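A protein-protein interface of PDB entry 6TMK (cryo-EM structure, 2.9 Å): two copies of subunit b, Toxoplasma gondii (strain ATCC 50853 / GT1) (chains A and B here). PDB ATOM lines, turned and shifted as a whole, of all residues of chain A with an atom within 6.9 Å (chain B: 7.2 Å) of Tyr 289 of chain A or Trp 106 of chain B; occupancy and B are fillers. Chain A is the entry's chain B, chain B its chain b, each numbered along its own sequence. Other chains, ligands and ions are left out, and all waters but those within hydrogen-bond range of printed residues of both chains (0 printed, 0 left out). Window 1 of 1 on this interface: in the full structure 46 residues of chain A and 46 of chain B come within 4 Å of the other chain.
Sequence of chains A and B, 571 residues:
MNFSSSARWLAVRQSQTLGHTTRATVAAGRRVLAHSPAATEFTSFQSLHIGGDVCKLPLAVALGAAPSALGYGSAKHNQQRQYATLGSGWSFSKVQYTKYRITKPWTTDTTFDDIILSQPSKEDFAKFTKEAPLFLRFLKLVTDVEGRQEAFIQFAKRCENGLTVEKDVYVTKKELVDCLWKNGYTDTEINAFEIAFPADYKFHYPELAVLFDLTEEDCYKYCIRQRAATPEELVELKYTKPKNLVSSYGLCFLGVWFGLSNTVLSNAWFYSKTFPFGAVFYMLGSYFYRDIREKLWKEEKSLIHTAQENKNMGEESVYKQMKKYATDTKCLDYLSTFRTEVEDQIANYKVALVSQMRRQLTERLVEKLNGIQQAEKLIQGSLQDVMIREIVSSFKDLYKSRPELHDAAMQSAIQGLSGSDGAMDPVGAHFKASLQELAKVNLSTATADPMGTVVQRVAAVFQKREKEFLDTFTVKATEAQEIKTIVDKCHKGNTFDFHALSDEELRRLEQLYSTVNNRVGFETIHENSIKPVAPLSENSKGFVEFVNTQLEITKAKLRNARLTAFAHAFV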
ATOM      1  N   SER A  93      21.264  31.304  18.889  1.00  0.00           N
ATOM      2  CA  SER A  93      20.869  30.152  19.682  1.00  0.00           C
ATOM      3  C   SER A  93      19.385  30.220  19.994  1.00  0.00           C
ATOM      4  O   SER A  93      18.896  31.228  20.512  1.00  0.00           O
ATOM      5  CB  SER A  93      21.663  30.078  20.984  1.00  0.00           C
ATOM      6  OG  SER A  93      21.232  28.985  21.772  1.00  0.00           O
ATOM      7  N   LYS A  94      18.680  29.146  19.670  1.00  0.00           N
ATOM      8  CA  LYS A  94      17.295  28.952  20.050  1.00  0.00           C
ATOM      9  C   LYS A  94      17.194  27.649  20.825  1.00  0.00           C
ATOM     10  O   LYS A  94      18.110  26.824  20.809  1.00  0.00           O
ATOM     11  CB  LYS A  94      16.383  28.943  18.821  1.00  0.00           C
ATOM     12  CG  LYS A  94      16.320  30.283  18.122  1.00  0.00           C
ATOM     13  CD  LYS A  94      15.452  31.265  18.868  1.00  0.00           C
ATOM     14  CE  LYS A  94      15.203  32.509  18.056  1.00  0.00           C
ATOM     15  NZ  LYS A  94      14.578  33.576  18.877  1.00  0.00           N
ATOM     16  N   VAL A  95      16.073  27.468  21.510  1.00  0.00           N
ATOM     17  CA  VAL A  95      15.891  26.339  22.410  1.00  0.00           C
ATOM     18  C   VAL A  95      14.614  25.603  22.056  1.00  0.00           C
ATOM     19  O   VAL A  95      13.650  26.188  21.552  1.00  0.00           O
ATOM     20  CB  VAL A  95      15.854  26.773  23.889  1.00  0.00           C
ATOM     21  CG1 VAL A  95      17.188  27.288  24.319  1.00  0.00           C
ATOM     22  CG2 VAL A  95      14.782  27.815  24.123  1.00  0.00           C
ATOM     23  N   GLN A  96      14.620  24.304  22.322  1.00  0.00           N
ATOM     24  CA  GLN A  96      13.426  23.478  22.300  1.00  0.00           C
ATOM     25  C   GLN A  96      13.138  23.004  23.715  1.00  0.00           C
ATOM     26  O   GLN A  96      14.059  22.745  24.494  1.00  0.00           O
ATOM     27  CB  GLN A  96      13.596  22.278  21.372  1.00  0.00           C
ATOM     28  CG  GLN A  96      14.811  21.452  21.655  1.00  0.00           C
ATOM     29  CD  GLN A  96      14.792  20.134  20.931  1.00  0.00           C
ATOM     30  OE1 GLN A  96      13.761  19.471  20.849  1.00  0.00           O
ATOM     31  NE2 GLN A  96      15.930  19.749  20.387  1.00  0.00           N
ATOM     32  N   TYR A  97      11.862  22.897  24.040  1.00  0.00           N
ATOM     33  CA  TYR A  97      11.435  22.535  25.379  1.00  0.00           C
ATOM     34  C   TYR A  97      11.046  21.066  25.445  1.00  0.00           C
ATOM     35  O   TYR A  97      10.721  20.431  24.441  1.00  0.00           O
ATOM     36  CB  TYR A  97      10.259  23.402  25.833  1.00  0.00           C
ATOM     37  CG  TYR A  97       9.007  23.251  25.015  1.00  0.00           C
ATOM     38  CD1 TYR A  97       8.049  22.320  25.361  1.00  0.00           C
ATOM     39  CD2 TYR A  97       8.770  24.044  23.914  1.00  0.00           C
ATOM     40  CE1 TYR A  97       6.914  22.169  24.630  1.00  0.00           C
ATOM     41  CE2 TYR A  97       7.627  23.899  23.177  1.00  0.00           C
ATOM     42  CZ  TYR A  97       6.699  22.959  23.545  1.00  0.00           C
ATOM     43  OH  TYR A  97       5.546  22.784  22.829  1.00  0.00           O
ATOM     44  N   MET A 283      -3.269  21.156  16.753  1.00  0.00           N
ATOM     45  CA  MET A 283      -2.772  20.018  15.992  1.00  0.00           C
ATOM     46  C   MET A 283      -1.800  20.464  14.914  1.00  0.00           C
ATOM     47  O   MET A 283      -0.748  19.843  14.720  1.00  0.00           O
ATOM     48  CB  MET A 283      -3.938  19.258  15.372  1.00  0.00           C
ATOM     49  CG  MET A 283      -4.714  18.394  16.339  1.00  0.00           C
ATOM     50  SD  MET A 283      -5.727  17.161  15.508  1.00  0.00           S
ATOM     51  CE  MET A 283      -6.747  18.200  14.467  1.00  0.00           C
ATOM     52  N   LEU A 284      -2.124  21.544  14.207  1.00  0.00           N
ATOM     53  CA  LEU A 284      -1.226  22.035  13.174  1.00  0.00           C
ATOM     54  C   LEU A 284       0.078  22.534  13.771  1.00  0.00           C
ATOM     55  O   LEU A 284       1.151  22.288  13.213  1.00  0.00           O
ATOM     56  CB  LEU A 284      -1.901  23.146  12.379  1.00  0.00           C
ATOM     57  CG  LEU A 284      -3.084  22.751  11.502  1.00  0.00           C
ATOM     58  CD1 LEU A 284      -3.668  23.991  10.863  1.00  0.00           C
ATOM     59  CD2 LEU A 284      -2.690  21.743  10.455  1.00  0.00           C
ATOM     60  N   GLY A 285       0.013  23.246  14.895  1.00  0.00           N
ATOM     61  CA  GLY A 285       1.230  23.684  15.545  1.00  0.00           C
ATOM     62  C   GLY A 285       2.081  22.531  16.026  1.00  0.00           C
ATOM     63  O   GLY A 285       3.307  22.566  15.919  1.00  0.00           O
ATOM     64  N   SER A 286       1.446  21.489  16.555  1.00  0.00           N
ATOM     65  CA  SER A 286       2.196  20.332  17.019  1.00  0.00           C
ATOM     66  C   SER A 286       2.843  19.595  15.855  1.00  0.00           C
ATOM     67  O   SER A 286       3.964  19.091  15.980  1.00  0.00           O
ATOM     68  CB  SER A 286       1.277  19.411  17.812  1.00  0.00           C
ATOM     69  OG  SER A 286       1.969  18.272  18.280  1.00  0.00           O
ATOM     70  N   TYR A 287       2.160  19.529  14.713  1.00  0.00           N
ATOM     71  CA  TYR A 287       2.680  18.757  13.592  1.00  0.00           C
ATOM     72  C   TYR A 287       3.732  19.533  12.809  1.00  0.00           C
ATOM     73  O   TYR A 287       4.698  18.942  12.318  1.00  0.00           O
ATOM     74  CB  TYR A 287       1.537  18.324  12.675  1.00  0.00           C
ATOM     75  CG  TYR A 287       1.906  17.197  11.746  1.00  0.00           C
ATOM     76  CD1 TYR A 287       1.953  15.895  12.199  1.00  0.00           C
ATOM     77  CD2 TYR A 287       2.212  17.437  10.419  1.00  0.00           C
ATOM     78  CE1 TYR A 287       2.291  14.866  11.362  1.00  0.00           C
ATOM     79  CE2 TYR A 287       2.555  16.413   9.575  1.00  0.00           C
ATOM     80  CZ  TYR A 287       2.592  15.127  10.049  1.00  0.00           C
ATOM     81  OH  TYR A 287       2.935  14.097   9.208  1.00  0.00           O
ATOM     82  N   PHE A 288       3.566  20.846  12.678  1.00  0.00           N
ATOM     83  CA  PHE A 288       4.498  21.701  11.956  1.00  0.00           C
ATOM     84  C   PHE A 288       5.205  22.664  12.902  1.00  0.00           C
ATOM     85  O   PHE A 288       5.485  23.810  12.551  1.00  0.00           O
ATOM     86  CB  PHE A 288       3.776  22.478  10.863  1.00  0.00           C
ATOM     87  CG  PHE A 288       3.038  21.617   9.892  1.00  0.00           C
ATOM     88  CD1 PHE A 288       1.663  21.566   9.905  1.00  0.00           C
ATOM     89  CD2 PHE A 288       3.716  20.861   8.962  1.00  0.00           C
ATOM     90  CE1 PHE A 288       0.982  20.780   9.018  1.00  0.00           C
ATOM     91  CE2 PHE A 288       3.037  20.074   8.070  1.00  0.00           C
ATOM     92  CZ  PHE A 288       1.666  20.035   8.097  1.00  0.00           C
ATOM     93  N   TYR A 289       5.517  22.198  14.109  1.00  0.00           N
ATOM     94  CA  TYR A 289       6.174  23.047  15.091  1.00  0.00           C
ATOM     95  C   TYR A 289       7.508  23.551  14.564  1.00  0.00           C
ATOM     96  O   TYR A 289       7.830  24.736  14.689  1.00  0.00           O
ATOM     97  CB  TYR A 289       6.353  22.281  16.400  1.00  0.00           C
ATOM     98  CG  TYR A 289       6.964  23.082  17.516  1.00  0.00           C
ATOM     99  CD1 TYR A 289       6.241  24.060  18.166  1.00  0.00           C
ATOM    100  CD2 TYR A 289       8.261  22.853  17.930  1.00  0.00           C
ATOM    101  CE1 TYR A 289       6.789  24.789  19.182  1.00  0.00           C
ATOM    102  CE2 TYR A 289       8.820  23.584  18.948  1.00  0.00           C
ATOM    103  CZ  TYR A 289       8.079  24.551  19.571  1.00  0.00           C
ATOM    104  OH  TYR A 289       8.632  25.283  20.591  1.00  0.00           O
ATOM    105  N   ARG A 290       8.300  22.662  13.973  1.00  0.00           N
ATOM    106  CA  ARG A 290       9.660  22.990  13.584  1.00  0.00           C
ATOM    107  C   ARG A 290       9.736  23.614  12.198  1.00  0.00           C
ATOM    108  O   ARG A 290      10.563  24.504  11.964  1.00  0.00           O
ATOM    109  CB  ARG A 290      10.503  21.722  13.627  1.00  0.00           C
ATOM    110  CG  ARG A 290      10.247  20.905  14.857  1.00  0.00           C
ATOM    111  CD  ARG A 290      11.432  20.092  15.271  1.00  0.00           C
ATOM    112  NE  ARG A 290      11.367  19.745  16.685  1.00  0.00           N
ATOM    113  CZ  ARG A 290      12.309  19.074  17.333  1.00  0.00           C
ATOM    114  NH1 ARG A 290      13.397  18.674  16.707  1.00  0.00           N
ATOM    115  NH2 ARG A 290      12.158  18.807  18.613  1.00  0.00           N
ATOM    116  N   ASP A 291       8.885  23.167  11.275  1.00  0.00           N
ATOM    117  CA  ASP A 291       8.831  23.772   9.950  1.00  0.00           C
ATOM    118  C   ASP A 291       8.576  25.268  10.050  1.00  0.00           C
ATOM    119  O   ASP A 291       9.245  26.076   9.395  1.00  0.00           O
ATOM    120  CB  ASP A 291       7.743  23.098   9.123  1.00  0.00           C
ATOM    121  CG  ASP A 291       7.939  21.603   9.005  1.00  0.00           C
ATOM    122  OD1 ASP A 291       7.643  20.885   9.984  1.00  0.00           O
ATOM    123  OD2 ASP A 291       8.385  21.144   7.934  1.00  0.00           O
ATOM    124  N   ILE A 292       7.599  25.649  10.871  1.00  0.00           N
ATOM    125  CA  ILE A 292       7.233  27.051  11.024  1.00  0.00           C
ATOM    126  C   ILE A 292       8.408  27.844  11.578  1.00  0.00           C
ATOM    127  O   ILE A 292       8.766  28.909  11.060  1.00  0.00           O
ATOM    128  CB  ILE A 292       5.993  27.174  11.928  1.00  0.00           C
ATOM    129  CG1 ILE A 292       4.770  26.593  11.231  1.00  0.00           C
ATOM    130  CG2 ILE A 292       5.737  28.618  12.297  1.00  0.00           C
ATOM    131  CD1 ILE A 292       3.656  26.238  12.170  1.00  0.00           C
ATOM    132  N   ARG A 293       9.008  27.346  12.660  1.00  0.00           N
ATOM    133  CA  ARG A 293      10.097  28.076  13.292  1.00  0.00           C
ATOM    134  C   ARG A 293      11.259  28.257  12.327  1.00  0.00           C
ATOM    135  O   ARG A 293      11.868  29.331  12.270  1.00  0.00           O
ATOM    136  CB  ARG A 293      10.565  27.331  14.537  1.00  0.00           C
ATOM    137  CG  ARG A 293       9.528  27.162  15.621  1.00  0.00           C
ATOM    138  CD  ARG A 293       9.116  28.473  16.195  1.00  0.00           C
ATOM    139  NE  ARG A 293       8.350  28.338  17.431  1.00  0.00           N
ATOM    140  CZ  ARG A 293       7.118  27.847  17.501  1.00  0.00           C
ATOM    141  NH1 ARG A 293       6.495  27.424  16.416  1.00  0.00           N
ATOM    142  NH2 ARG A 293       6.506  27.779  18.665  1.00  0.00           N
ATOM    143  N   GLU A 294      11.578  27.219  11.556  1.00  0.00           N
ATOM    144  CA  GLU A 294      12.677  27.312  10.606  1.00  0.00           C
ATOM    145  C   GLU A 294      12.373  28.319   9.505  1.00  0.00           C
ATOM    146  O   GLU A 294      13.225  29.144   9.144  1.00  0.00           O
ATOM    147  CB  GLU A 294      12.951  25.937  10.017  1.00  0.00           C
ATOM    148  CG  GLU A 294      13.516  24.971  11.019  1.00  0.00           C
ATOM    149  CD  GLU A 294      13.287  23.528  10.629  1.00  0.00           C
ATOM    150  OE1 GLU A 294      13.037  23.266   9.434  1.00  0.00           O
ATOM    151  OE2 GLU A 294      13.355  22.654  11.520  1.00  0.00           O
ATOM    152  N   TRP A 297      12.847  31.763  11.022  1.00  0.00           N
ATOM    153  CA  TRP A 297      14.197  32.121  11.437  1.00  0.00           C
ATOM    154  C   TRP A 297      15.209  32.122  10.302  1.00  0.00           C
ATOM    155  O   TRP A 297      16.360  32.520  10.525  1.00  0.00           O
ATOM    156  CB  TRP A 297      14.673  31.159  12.517  1.00  0.00           C
ATOM    157  CG  TRP A 297      13.829  31.138  13.728  1.00  0.00           C
ATOM    158  CD1 TRP A 297      12.973  32.104  14.143  1.00  0.00           C
ATOM    159  CD2 TRP A 297      13.755  30.095  14.696  1.00  0.00           C
ATOM    160  NE1 TRP A 297      12.369  31.731  15.312  1.00  0.00           N
ATOM    161  CE2 TRP A 297      12.834  30.498  15.673  1.00  0.00           C
ATOM    162  CE3 TRP A 297      14.382  28.856  14.833  1.00  0.00           C
ATOM    163  CZ2 TRP A 297      12.526  29.711  16.768  1.00  0.00           C
ATOM    164  CZ3 TRP A 297      14.071  28.082  15.916  1.00  0.00           C
ATOM    165  CH2 TRP A 297      13.152  28.510  16.871  1.00  0.00           C
ATOM    166  N   LYS B 104      16.784  22.567  25.742  1.00  0.00           N
ATOM    167  CA  LYS B 104      17.963  22.106  25.041  1.00  0.00           C
ATOM    168  C   LYS B 104      18.097  22.878  23.740  1.00  0.00           C
ATOM    169  O   LYS B 104      17.142  23.522  23.290  1.00  0.00           O
ATOM    170  CB  LYS B 104      17.873  20.604  24.752  1.00  0.00           C
ATOM    171  CG  LYS B 104      17.820  19.758  25.994  1.00  0.00           C
ATOM    172  CD  LYS B 104      19.161  19.672  26.667  1.00  0.00           C
ATOM    173  CE  LYS B 104      19.166  18.596  27.707  1.00  0.00           C
ATOM    174  NZ  LYS B 104      20.121  18.882  28.798  1.00  0.00           N
ATOM    175  N   PRO B 105      19.270  22.859  23.119  1.00  0.00           N
ATOM    176  CA  PRO B 105      19.456  23.639  21.895  1.00  0.00           C
ATOM    177  C   PRO B 105      18.568  23.134  20.773  1.00  0.00           C
ATOM    178  O   PRO B 105      18.248  21.947  20.684  1.00  0.00           O
ATOM    179  CB  PRO B 105      20.939  23.446  21.574  1.00  0.00           C
ATOM    180  CG  PRO B 105      21.548  23.029  22.846  1.00  0.00           C
ATOM    181  CD  PRO B 105      20.521  22.217  23.538  1.00  0.00           C
ATOM    182  N   TRP B 106      18.176  24.061  19.908  1.00  0.00           N
ATOM    183  CA  TRP B 106      17.279  23.737  18.812  1.00  0.00           C
ATOM    184  C   TRP B 106      17.913  22.753  17.842  1.00  0.00           C
ATOM    185  O   TRP B 106      19.075  22.896  17.453  1.00  0.00           O
ATOM    186  CB  TRP B 106      16.881  25.006  18.070  1.00  0.00           C
ATOM    187  CG  TRP B 106      15.936  24.745  16.964  1.00  0.00           C
ATOM    188  CD1 TRP B 106      16.235  24.578  15.650  1.00  0.00           C
ATOM    189  CD2 TRP B 106      14.521  24.605  17.075  1.00  0.00           C
ATOM    190  NE1 TRP B 106      15.094  24.348  14.932  1.00  0.00           N
ATOM    191  CE2 TRP B 106      14.025  24.359  15.786  1.00  0.00           C
ATOM    192  CE3 TRP B 106      13.625  24.669  18.140  1.00  0.00           C
ATOM    193  CZ2 TRP B 106      12.677  24.176  15.535  1.00  0.00           C
ATOM    194  CZ3 TRP B 106      12.296  24.487  17.890  1.00  0.00           C
ATOM    195  CH2 TRP B 106      11.829  24.243  16.598  1.00  0.00           C
ATOM    196  N   THR B 107      17.136  21.746  17.461  1.00  0.00           N
ATOM    197  CA  THR B 107      17.497  20.823  16.401  1.00  0.00           C
ATOM    198  C   THR B 107      16.244  20.474  15.617  1.00  0.00           C
ATOM    199  O   THR B 107      15.160  20.341  16.190  1.00  0.00           O
ATOM    200  CB  THR B 107      18.134  19.544  16.942  1.00  0.00           C
ATOM    201  OG1 THR B 107      17.239  18.912  17.863  1.00  0.00           O
ATOM    202  CG2 THR B 107      19.431  19.852  17.639  1.00  0.00           C
ATOM    203  N   THR B 108      16.400  20.329  14.308  1.00  0.00           N
ATOM    204  CA  THR B 108      15.280  20.050  13.426  1.00  0.00           C
ATOM    205  C   THR B 108      15.000  18.562  13.287  1.00  0.00           C
ATOM    206  O   THR B 108      13.972  18.191  12.712  1.00  0.00           O
ATOM    207  CB  THR B 108      15.530  20.650  12.039  1.00  0.00           C
ATOM    208  OG1 THR B 108      14.440  20.319  11.173  1.00  0.00           O
ATOM    209  CG2 THR B 108      16.833  20.130  11.449  1.00  0.00           C
ATOM    210  N   ASP B 109      15.882  17.708  13.804  1.00  0.00           N
ATOM    211  CA  ASP B 109      15.776  16.268  13.634  1.00  0.00           C
ATOM    212  C   ASP B 109      15.786  15.490  14.936  1.00  0.00           C
ATOM    213  O   ASP B 109      15.393  14.317  14.925  1.00  0.00           O
ATOM    214  CB  ASP B 109      16.921  15.748  12.756  1.00  0.00           C
ATOM    215  CG  ASP B 109      18.271  16.272  13.194  1.00  0.00           C
ATOM    216  OD1 ASP B 109      18.302  17.190  14.039  1.00  0.00           O
ATOM    217  OD2 ASP B 109      19.300  15.764  12.702  1.00  0.00           O
ATOM    218  N   THR B 110      16.217  16.078  16.045  1.00  0.00           N
ATOM    219  CA  THR B 110      16.357  15.357  17.296  1.00  0.00           C
ATOM    220  C   THR B 110      15.431  15.931  18.357  1.00  0.00           C
ATOM    221  O   THR B 110      14.963  17.068  18.266  1.00  0.00           O
ATOM    222  CB  THR B 110      17.796  15.406  17.810  1.00  0.00           C
ATOM    223  OG1 THR B 110      18.135  16.749  18.169  1.00  0.00           O
ATOM    224  CG2 THR B 110      18.745  14.927  16.756  1.00  0.00           C
ATOM    225  N   PHE B 112      14.922  15.498  22.880  1.00  0.00           N
ATOM    226  CA  PHE B 112      15.478  14.990  24.124  1.00  0.00           C
ATOM    227  C   PHE B 112      14.394  14.379  24.997  1.00  0.00           C
ATOM    228  O   PHE B 112      13.288  14.918  25.100  1.00  0.00           O
ATOM    229  CB  PHE B 112      16.192  16.101  24.878  1.00  0.00           C
ATOM    230  CG  PHE B 112      17.454  16.546  24.230  1.00  0.00           C
ATOM    231  CD1 PHE B 112      18.673  16.115  24.701  1.00  0.00           C
ATOM    232  CD2 PHE B 112      17.424  17.398  23.149  1.00  0.00           C
ATOM    233  CE1 PHE B 112      19.833  16.523  24.107  1.00  0.00           C
ATOM    234  CE2 PHE B 112      18.582  17.809  22.553  1.00  0.00           C
ATOM    235  CZ  PHE B 112      19.787  17.375  23.030  1.00  0.00           C
ATOM    236  N   TYR B 239      13.728  12.698  16.061  1.00  0.00           N
ATOM    237  CA  TYR B 239      12.433  13.359  16.127  1.00  0.00           C
ATOM    238  C   TYR B 239      11.422  12.622  15.265  1.00  0.00           C
ATOM    239  O   TYR B 239      11.703  12.274  14.115  1.00  0.00           O
ATOM    240  CB  TYR B 239      12.551  14.808  15.671  1.00  0.00           C
ATOM    241  CG  TYR B 239      11.252  15.572  15.703  1.00  0.00           C
ATOM    242  CD1 TYR B 239      10.623  15.846  16.903  1.00  0.00           C
ATOM    243  CD2 TYR B 239      10.660  16.027  14.537  1.00  0.00           C
ATOM    244  CE1 TYR B 239       9.439  16.545  16.942  1.00  0.00           C
ATOM    245  CE2 TYR B 239       9.479  16.724  14.568  1.00  0.00           C
ATOM    246  CZ  TYR B 239       8.873  16.984  15.772  1.00  0.00           C
ATOM    247  OH  TYR B 239       7.689  17.684  15.811  1.00  0.00           O
ATOM    248  N   LYS B 241       7.155  12.808  14.191  1.00  0.00           N
ATOM    249  CA  LYS B 241       5.952  13.608  14.241  1.00  0.00           C
ATOM    250  C   LYS B 241       4.937  12.959  15.176  1.00  0.00           C
ATOM    251  O   LYS B 241       5.022  11.763  15.466  1.00  0.00           O
ATOM    252  CB  LYS B 241       5.351  13.755  12.850  1.00  0.00           C
ATOM    253  CG  LYS B 241       6.224  14.487  11.867  1.00  0.00           C
ATOM    254  CD  LYS B 241       6.251  15.962  12.142  1.00  0.00           C
ATOM    255  CE  LYS B 241       6.835  16.716  10.978  1.00  0.00           C
ATOM    256  NZ  LYS B 241       5.866  16.835   9.867  1.00  0.00           N
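OG1 of Thr 107 of chain B is in hydrogen-bond range of O of Thr 110 of chain B (3.0 Å).
The backbone NH (N) of Tyr 239 of chain B sits at hydrogen-bond distance from the backbone carbonyl oxygen (O) of Asp 109 of chain B (2.6 Å).
NH2 of Arg 290 of chain A lies within hydrogen-bond range of OE1 of Gln 96 of chain A, 2.8 Å away.
The backbone carbonyl oxygen (O) of Tyr 289 of chain A lies close to the guanidinium group (NH1) of Arg 293 of chain A (3.5 Å).
Ser 93 of chain A touches none of the printed residues of chain B.
Tyr 289 of chain A touches just one residue of chain B: Trp 106 (3.7 Å).
Of the printed residues of chain B, Trp 297 of chain A touches Trp 106.
Printed residues of chain A within 4 Å of Trp 106 of chain B: Lys 94, Val 95, Tyr 289, Arg 290, Arg 293 and Trp 297.
Printed residues of chain A within 4 Å of Lys 241 of chain B: Tyr 287 (3.4 Å).
The nearest printed residue of chain A that does not touch Thr 110 of chain B is Tyr 97 of chain A (8.2 Å).
The backbone carbonyl oxygen (O) of Lys 104 of chain B is in hydrogen-bond range of the backbone NH (N) of Gln 96 of chain A (2.8 Å).
The backbone carbonyl oxygen (O) of Pro 105 of chain B lies within hydrogen-bond range of the side-chain amide nitrogen (NE2) of Gln 96 of chain A, 3.2 Å away.
The backbone NH (N) of Trp 106 of chain B is in hydrogen-bond range of the backbone carbonyl oxygen (O) of Lys 94 of chain A.
The side-chain amide nitrogen of Gln 96 of chain A is in hydrogen-bond range of the side-chain hydroxyl of Thr 107 of chain B.
NH1 of Arg 290 of chain A sits at hydrogen-bond distance from O of Thr 107 of chain B.
OG1 of Thr 108 of chain B lies within hydrogen-bond range of OE2 of Glu 294 of chain A, at 2.6 Å.
The backbone carbonyl oxygen (O) of Thr 110 of chain B lies within hydrogen-bond range of the guanidinium group (NH1) of Arg 290 of chain A (2.7 Å).
O of Tyr 287 of chain A sits close to NZ of Lys 241 of chain B (3.4 Å).
Of the 10 printed residues of chain B, 10 touch a printed residue of chain A.
Hydrophobic or aromatic side chains of chain B that line the printed part of chain A: Trp 106, Phe 112 and Tyr 239.
Of the 18 printed residues of chain A, 10 touch a printed residue of chain B.
Hydrophobic or aromatic side chains of chain A within 4 Å of the printed part of chain B: Val 95, Tyr 287, Tyr 289 and Trp 297.
Among the printed residues, no Asp or Glu carboxylate lies within 4 Å of a Lys or Arg side-chain nitrogen of the other chain.
Lys 94 of chain A touches Pro 105 of chain B (O to CA, 3.6 Å).
Val 95 of chain A touches Lys 104 of chain B (CA to O, 3.2 Å).
Trp 106 of chain B touches Val 95 of chain A (CE3 to O, 3.7 Å).
Gln 96 of chain A touches Thr 110 of chain B.
CE2 of Tyr 289 of chain A touches CZ3 of Trp 106 of chain B, 3.7 Å away.
Trp 106 of chain B touches Arg 290 of chain A.
NH1 of Arg 290 of chain A touches C of Thr 108 of chain B, 3.8 Å away.
Asp 109 of chain B touches Arg 290 of chain A (N to NH1, 3.9 Å).
Trp 106 of chain B touches Arg 293 of chain A (CH2 to CG, 3.8 Å).
Trp 297 of chain A touches Trp 106 of chain B (CZ3 to CD2, 3.7 Å).
No position is printed for both chains.
Of the 21 pairs that touch across the chains among the printed residues, none has its exchanged pair printed and touching as well.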
